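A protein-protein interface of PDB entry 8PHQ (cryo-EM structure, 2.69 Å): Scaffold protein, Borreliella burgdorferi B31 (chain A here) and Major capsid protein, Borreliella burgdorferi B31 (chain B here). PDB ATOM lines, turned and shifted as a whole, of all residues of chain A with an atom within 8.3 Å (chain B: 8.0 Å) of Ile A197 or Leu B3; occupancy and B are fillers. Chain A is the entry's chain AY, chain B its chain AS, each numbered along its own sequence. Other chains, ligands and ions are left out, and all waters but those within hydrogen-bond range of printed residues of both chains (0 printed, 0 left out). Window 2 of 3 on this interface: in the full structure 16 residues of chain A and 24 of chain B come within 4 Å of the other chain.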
ATOM      1  N   PHE A 194      19.127  10.266   7.212  1.00  0.00           N
ATOM      2  CA  PHE A 194      18.232  11.386   7.463  1.00  0.00           C
ATOM      3  C   PHE A 194      17.244  11.567   6.318  1.00  0.00           C
ATOM      4  O   PHE A 194      17.615  11.527   5.141  1.00  0.00           O
ATOM      5  CB  PHE A 194      19.031  12.672   7.665  1.00  0.00           C
ATOM      6  CG  PHE A 194      18.191  13.916   7.641  1.00  0.00           C
ATOM      7  CD1 PHE A 194      17.286  14.176   8.656  1.00  0.00           C
ATOM      8  CD2 PHE A 194      18.294  14.817   6.595  1.00  0.00           C
ATOM      9  CE1 PHE A 194      16.509  15.318   8.636  1.00  0.00           C
ATOM     10  CE2 PHE A 194      17.518  15.959   6.569  1.00  0.00           C
ATOM     11  CZ  PHE A 194      16.626  16.211   7.592  1.00  0.00           C
ATOM     12  N   VAL A 195      15.979  11.770   6.672  1.00  0.00           N
ATOM     13  CA  VAL A 195      14.929  12.076   5.704  1.00  0.00           C
ATOM     14  C   VAL A 195      14.119  13.248   6.247  1.00  0.00           C
ATOM     15  O   VAL A 195      13.411  13.098   7.253  1.00  0.00           O
ATOM     16  CB  VAL A 195      14.036  10.855   5.433  1.00  0.00           C
ATOM     17  CG1 VAL A 195      12.781  11.270   4.678  1.00  0.00           C
ATOM     18  CG2 VAL A 195      14.801   9.802   4.649  1.00  0.00           C
ATOM     19  N   PRO A 196      14.205  14.426   5.635  1.00  0.00           N
ATOM     20  CA  PRO A 196      13.449  15.574   6.145  1.00  0.00           C
ATOM     21  C   PRO A 196      11.955  15.387   5.952  1.00  0.00           C
ATOM     22  O   PRO A 196      11.500  14.710   5.026  1.00  0.00           O
ATOM     23  CB  PRO A 196      13.973  16.744   5.308  1.00  0.00           C
ATOM     24  CG  PRO A 196      14.461  16.116   4.053  1.00  0.00           C
ATOM     25  CD  PRO A 196      14.993  14.766   4.438  1.00  0.00           C
ATOM     26  N   ILE A 197      11.188  16.005   6.844  1.00  0.00           N
ATOM     27  CA  ILE A 197       9.736  16.002   6.712  1.00  0.00           C
ATOM     28  C   ILE A 197       9.255  17.216   5.929  1.00  0.00           C
ATOM     29  O   ILE A 197       8.382  17.096   5.066  1.00  0.00           O
ATOM     30  CB  ILE A 197       9.073  15.931   8.101  1.00  0.00           C
ATOM     31  CG1 ILE A 197       9.497  14.657   8.832  1.00  0.00           C
ATOM     32  CG2 ILE A 197       7.558  15.988   7.975  1.00  0.00           C
ATOM     33  CD1 ILE A 197       8.879  14.507  10.205  1.00  0.00           C
ATOM     34  N   ASN A 198       9.811  18.394   6.205  1.00  0.00           N
ATOM     35  CA  ASN A 198       9.385  19.620   5.551  1.00  0.00           C
ATOM     36  C   ASN A 198      10.595  20.467   5.167  1.00  0.00           C
ATOM     37  O   ASN A 198      11.751  20.145   5.477  1.00  0.00           O
ATOM     38  CB  ASN A 198       8.422  20.410   6.448  1.00  0.00           C
ATOM     39  CG  ASN A 198       8.966  20.617   7.845  1.00  0.00           C
ATOM     40  OD1 ASN A 198       9.994  21.265   8.035  1.00  0.00           O
ATOM     41  ND2 ASN A 198       8.276  20.062   8.833  1.00  0.00           N
ATOM     42  N   PHE A 199      10.302  21.580   4.489  1.00  0.00           N
ATOM     43  CA  PHE A 199      11.351  22.444   3.967  1.00  0.00           C
ATOM     44  C   PHE A 199      12.143  23.106   5.088  1.00  0.00           C
ATOM     45  O   PHE A 199      13.335  23.385   4.921  1.00  0.00           O
ATOM     46  CB  PHE A 199      10.740  23.501   3.046  1.00  0.00           C
ATOM     47  CG  PHE A 199      11.710  24.084   2.062  1.00  0.00           C
ATOM     48  CD1 PHE A 199      12.223  23.311   1.037  1.00  0.00           C
ATOM     49  CD2 PHE A 199      12.115  25.402   2.166  1.00  0.00           C
ATOM     50  CE1 PHE A 199      13.116  23.842   0.129  1.00  0.00           C
ATOM     51  CE2 PHE A 199      13.010  25.939   1.263  1.00  0.00           C
ATOM     52  CZ  PHE A 199      13.511  25.156   0.242  1.00  0.00           C
ATOM     53  N   THR A 200      11.504  23.363   6.232  1.00  0.00           N
ATOM     54  CA  THR A 200      12.224  23.921   7.373  1.00  0.00           C
ATOM     55  C   THR A 200      13.296  22.958   7.869  1.00  0.00           C
ATOM     56  O   THR A 200      14.445  23.354   8.115  1.00  0.00           O
ATOM     57  CB  THR A 200      11.245  24.252   8.499  1.00  0.00           C
ATOM     58  OG1 THR A 200      10.282  25.205   8.033  1.00  0.00           O
ATOM     59  CG2 THR A 200      11.987  24.816   9.697  1.00  0.00           C
ATOM     60  N   GLU A 201      12.936  21.683   8.025  1.00  0.00           N
ATOM     61  CA  GLU A 201      13.920  20.683   8.417  1.00  0.00           C
ATOM     62  C   GLU A 201      14.999  20.530   7.357  1.00  0.00           C
ATOM     63  O   GLU A 201      16.170  20.316   7.689  1.00  0.00           O
ATOM     64  CB  GLU A 201      13.228  19.347   8.681  1.00  0.00           C
ATOM     65  CG  GLU A 201      12.192  19.411   9.789  1.00  0.00           C
ATOM     66  CD  GLU A 201      11.508  18.082  10.027  1.00  0.00           C
ATOM     67  OE1 GLU A 201      11.875  17.094   9.356  1.00  0.00           O
ATOM     68  OE2 GLU A 201      10.602  18.023  10.885  1.00  0.00           O
ATOM     69  N   PHE A 202      14.630  20.662   6.081  1.00  0.00           N
ATOM     70  CA  PHE A 202      15.631  20.625   5.020  1.00  0.00           C
ATOM     71  C   PHE A 202      16.632  21.770   5.165  1.00  0.00           C
ATOM     72  O   PHE A 202      17.847  21.573   5.012  1.00  0.00           O
ATOM     73  CB  PHE A 202      14.929  20.671   3.663  1.00  0.00           C
ATOM     74  CG  PHE A 202      15.860  20.655   2.491  1.00  0.00           C
ATOM     75  CD1 PHE A 202      16.752  19.615   2.311  1.00  0.00           C
ATOM     76  CD2 PHE A 202      15.820  21.669   1.548  1.00  0.00           C
ATOM     77  CE1 PHE A 202      17.600  19.595   1.227  1.00  0.00           C
ATOM     78  CE2 PHE A 202      16.664  21.651   0.462  1.00  0.00           C
ATOM     79  CZ  PHE A 202      17.555  20.614   0.301  1.00  0.00           C
ATOM     80  N   VAL A 203      16.142  22.971   5.480  1.00  0.00           N
ATOM     81  CA  VAL A 203      17.024  24.125   5.652  1.00  0.00           C
ATOM     82  C   VAL A 203      17.947  23.924   6.849  1.00  0.00           C
ATOM     83  O   VAL A 203      19.148  24.232   6.789  1.00  0.00           O
ATOM     84  CB  VAL A 203      16.189  25.413   5.784  1.00  0.00           C
ATOM     85  CG1 VAL A 203      17.058  26.569   6.249  1.00  0.00           C
ATOM     86  CG2 VAL A 203      15.526  25.746   4.461  1.00  0.00           C
ATOM     87  N   LEU B   3       8.888  14.756   1.979  1.00  0.00           N
ATOM     88  CA  LEU B   3       9.289  15.971   1.282  1.00  0.00           C
ATOM     89  C   LEU B   3      10.071  15.644   0.015  1.00  0.00           C
ATOM     90  O   LEU B   3       9.815  16.215  -1.046  1.00  0.00           O
ATOM     91  CB  LEU B   3      10.127  16.866   2.197  1.00  0.00           C
ATOM     92  CG  LEU B   3      10.931  17.967   1.503  1.00  0.00           C
ATOM     93  CD1 LEU B   3      10.015  19.087   1.040  1.00  0.00           C
ATOM     94  CD2 LEU B   3      12.018  18.505   2.418  1.00  0.00           C
ATOM     95  N   PHE B   4      11.027  14.721   0.134  1.00  0.00           N
ATOM     96  CA  PHE B   4      11.854  14.360  -1.012  1.00  0.00           C
ATOM     97  C   PHE B   4      11.044  13.673  -2.102  1.00  0.00           C
ATOM     98  O   PHE B   4      11.363  13.812  -3.289  1.00  0.00           O
ATOM     99  CB  PHE B   4      13.010  13.467  -0.563  1.00  0.00           C
ATOM    100  CG  PHE B   4      14.171  14.224   0.009  1.00  0.00           C
ATOM    101  CD1 PHE B   4      14.160  15.608   0.048  1.00  0.00           C
ATOM    102  CD2 PHE B   4      15.270  13.553   0.515  1.00  0.00           C
ATOM    103  CE1 PHE B   4      15.226  16.308   0.574  1.00  0.00           C
ATOM    104  CE2 PHE B   4      16.339  14.249   1.043  1.00  0.00           C
ATOM    105  CZ  PHE B   4      16.316  15.628   1.074  1.00  0.00           C
ATOM    106  N   ASP B   5      10.005  12.927  -1.726  1.00  0.00           N
ATOM    107  CA  ASP B   5       9.135  12.320  -2.727  1.00  0.00           C
ATOM    108  C   ASP B   5       8.393  13.385  -3.527  1.00  0.00           C
ATOM    109  O   ASP B   5       8.198  13.235  -4.738  1.00  0.00           O
ATOM    110  CB  ASP B   5       8.148  11.366  -2.056  1.00  0.00           C
ATOM    111  CG  ASP B   5       8.840  10.238  -1.320  1.00  0.00           C
ATOM    112  OD1 ASP B   5      10.086  10.171  -1.370  1.00  0.00           O
ATOM    113  OD2 ASP B   5       8.140   9.418  -0.692  1.00  0.00           O
ATOM    114  N   GLU B   6       7.972  14.460  -2.866  1.00  0.00           N
ATOM    115  CA  GLU B   6       7.238  15.531  -3.526  1.00  0.00           C
ATOM    116  C   GLU B   6       8.152  16.596  -4.122  1.00  0.00           C
ATOM    117  O   GLU B   6       7.905  17.060  -5.241  1.00  0.00           O
ATOM    118  CB  GLU B   6       6.262  16.178  -2.542  1.00  0.00           C
ATOM    119  CG  GLU B   6       5.429  15.180  -1.756  1.00  0.00           C
ATOM    120  CD  GLU B   6       4.509  15.849  -0.757  1.00  0.00           C
ATOM    121  OE1 GLU B   6       4.509  17.096  -0.691  1.00  0.00           O
ATOM    122  OE2 GLU B   6       3.787  15.130  -0.035  1.00  0.00           O
ATOM    123  N   ASN B   7       9.202  17.002  -3.406  1.00  0.00           N
ATOM    124  CA  ASN B   7      10.035  18.134  -3.814  1.00  0.00           C
ATOM    125  C   ASN B   7      11.297  17.621  -4.505  1.00  0.00           C
ATOM    126  O   ASN B   7      12.319  17.351  -3.859  1.00  0.00           O
ATOM    127  CB  ASN B   7      10.370  19.012  -2.614  1.00  0.00           C
ATOM    128  CG  ASN B   7      10.699  20.434  -3.012  1.00  0.00           C
ATOM    129  OD1 ASN B   7      11.599  20.675  -3.812  1.00  0.00           O
ATOM    130  ND2 ASN B   7       9.959  21.388  -2.457  1.00  0.00           N
ATOM    131  N   TYR B   8      11.228  17.526  -5.836  1.00  0.00           N
ATOM    132  CA  TYR B   8      12.388  17.112  -6.618  1.00  0.00           C
ATOM    133  C   TYR B   8      13.539  18.091  -6.457  1.00  0.00           C
ATOM    134  O   TYR B   8      14.704  17.686  -6.428  1.00  0.00           O
ATOM    135  CB  TYR B   8      12.022  16.995  -8.095  1.00  0.00           C
ATOM    136  CG  TYR B   8      13.210  17.172  -9.018  1.00  0.00           C
ATOM    137  CD1 TYR B   8      14.121  16.142  -9.219  1.00  0.00           C
ATOM    138  CD2 TYR B   8      13.443  18.383  -9.660  1.00  0.00           C
ATOM    139  CE1 TYR B   8      15.212  16.303 -10.056  1.00  0.00           C
ATOM    140  CE2 TYR B   8      14.531  18.553 -10.499  1.00  0.00           C
ATOM    141  CZ  TYR B   8      15.411  17.511 -10.691  1.00  0.00           C
ATOM    142  OH  TYR B   8      16.495  17.678 -11.522  1.00  0.00           O
ATOM    143  N   TYR B   9      13.236  19.389  -6.413  1.00  0.00           N
ATOM    144  CA  TYR B   9      14.293  20.386  -6.313  1.00  0.00           C
ATOM    145  C   TYR B   9      15.029  20.269  -4.983  1.00  0.00           C
ATOM    146  O   TYR B   9      16.261  20.371  -4.933  1.00  0.00           O
ATOM    147  CB  TYR B   9      13.699  21.779  -6.499  1.00  0.00           C
ATOM    148  CG  TYR B   9      13.046  21.957  -7.851  1.00  0.00           C
ATOM    149  CD1 TYR B   9      13.790  21.889  -9.018  1.00  0.00           C
ATOM    150  CD2 TYR B   9      11.679  22.168  -7.958  1.00  0.00           C
ATOM    151  CE1 TYR B   9      13.196  22.039 -10.254  1.00  0.00           C
ATOM    152  CE2 TYR B   9      11.075  22.319  -9.190  1.00  0.00           C
ATOM    153  CZ  TYR B   9      11.838  22.254 -10.333  1.00  0.00           C
ATOM    154  OH  TYR B   9      11.240  22.405 -11.560  1.00  0.00           O
ATOM    155  N   ALA B  10      14.289  20.034  -3.897  1.00  0.00           N
ATOM    156  CA  ALA B  10      14.926  19.784  -2.610  1.00  0.00           C
ATOM    157  C   ALA B  10      15.770  18.518  -2.655  1.00  0.00           C
ATOM    158  O   ALA B  10      16.886  18.485  -2.122  1.00  0.00           O
ATOM    159  CB  ALA B  10      13.872  19.687  -1.509  1.00  0.00           C
ATOM    160  N   LYS B  11      15.256  17.466  -3.298  1.00  0.00           N
ATOM    161  CA  LYS B  11      16.034  16.237  -3.435  1.00  0.00           C
ATOM    162  C   LYS B  11      17.336  16.486  -4.190  1.00  0.00           C
ATOM    163  O   LYS B  11      18.404  16.016  -3.778  1.00  0.00           O
ATOM    164  CB  LYS B  11      15.194  15.171  -4.143  1.00  0.00           C
ATOM    165  CG  LYS B  11      15.942  13.894  -4.476  1.00  0.00           C
ATOM    166  CD  LYS B  11      15.085  12.973  -5.334  1.00  0.00           C
ATOM    167  CE  LYS B  11      15.828  11.696  -5.699  1.00  0.00           C
ATOM    168  NZ  LYS B  11      15.029  10.816  -6.600  1.00  0.00           N
ATOM    169  N   GLU B 283      12.053  28.191  -1.171  1.00  0.00           N
ATOM    170  CA  GLU B 283      10.991  27.239  -1.476  1.00  0.00           C
ATOM    171  C   GLU B 283      10.232  27.614  -2.742  1.00  0.00           C
ATOM    172  O   GLU B 283       9.740  26.729  -3.451  1.00  0.00           O
ATOM    173  CB  GLU B 283      10.028  27.133  -0.295  1.00  0.00           C
ATOM    174  CG  GLU B 283       9.092  25.943  -0.373  1.00  0.00           C
ATOM    175  CD  GLU B 283       8.293  25.744   0.898  1.00  0.00           C
ATOM    176  OE1 GLU B 283       8.456  26.553   1.836  1.00  0.00           O
ATOM    177  OE2 GLU B 283       7.507  24.776   0.963  1.00  0.00           O
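The side-chain amide oxygen (OD1) of Asn B7 sits at hydrogen-bond distance from the backbone NH (N) of Ala B10, 2.8 Å away.
OE1 of Glu A201 sits at hydrogen-bond distance from N of Ile A197 (2.8 Å).
The side-chain amide oxygen (OD1) of Asn A198 is in hydrogen-bond range of the backbone NH (N) of Thr A200, 3.2 Å away.
The side-chain amide oxygen of Asn A198 lies within hydrogen-bond range of the backbone NH of Glu A201 (3.0 Å).
Leu B3 touches Pro A196.
CG of Pro A196 touches CZ of Phe B4, 3.5 Å away.
Ile A197 touches Leu B3 (O to CB, 3.4 Å).
Asn A198 touches Leu B3.
Glu B283 touches Phe A199 (N to CE2, 3.5 Å).
Leu B3 touches Phe A202 (CD2 to CB, 3.8 Å).
Ala B10 touches Phe A202 (O to CZ, 3.3 Å).
Phe A194 touches none of the printed residues of chain B.
Val A195 touches none of the printed residues of chain B.
Ile A197 touches just one residue of chain B: Leu B3 (3.4 Å).
Printed residues of chain B within 4 Å of Phe A199: Glu B283.
Printed residues of chain A within 4 Å of Glu B283: Phe A199.
The nearest printed residue of chain B that does not touch Pro A196 is Ala B10 (6.6 Å).
Hydrophobic or aromatic side chains of chain B within 4 Å of the printed part of chain A: Leu B3, Phe B4 and Ala B10.
Among the printed residues, no Asp or Glu carboxylate lies within 4 Å of a Lys or Arg side-chain nitrogen of the other chain.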
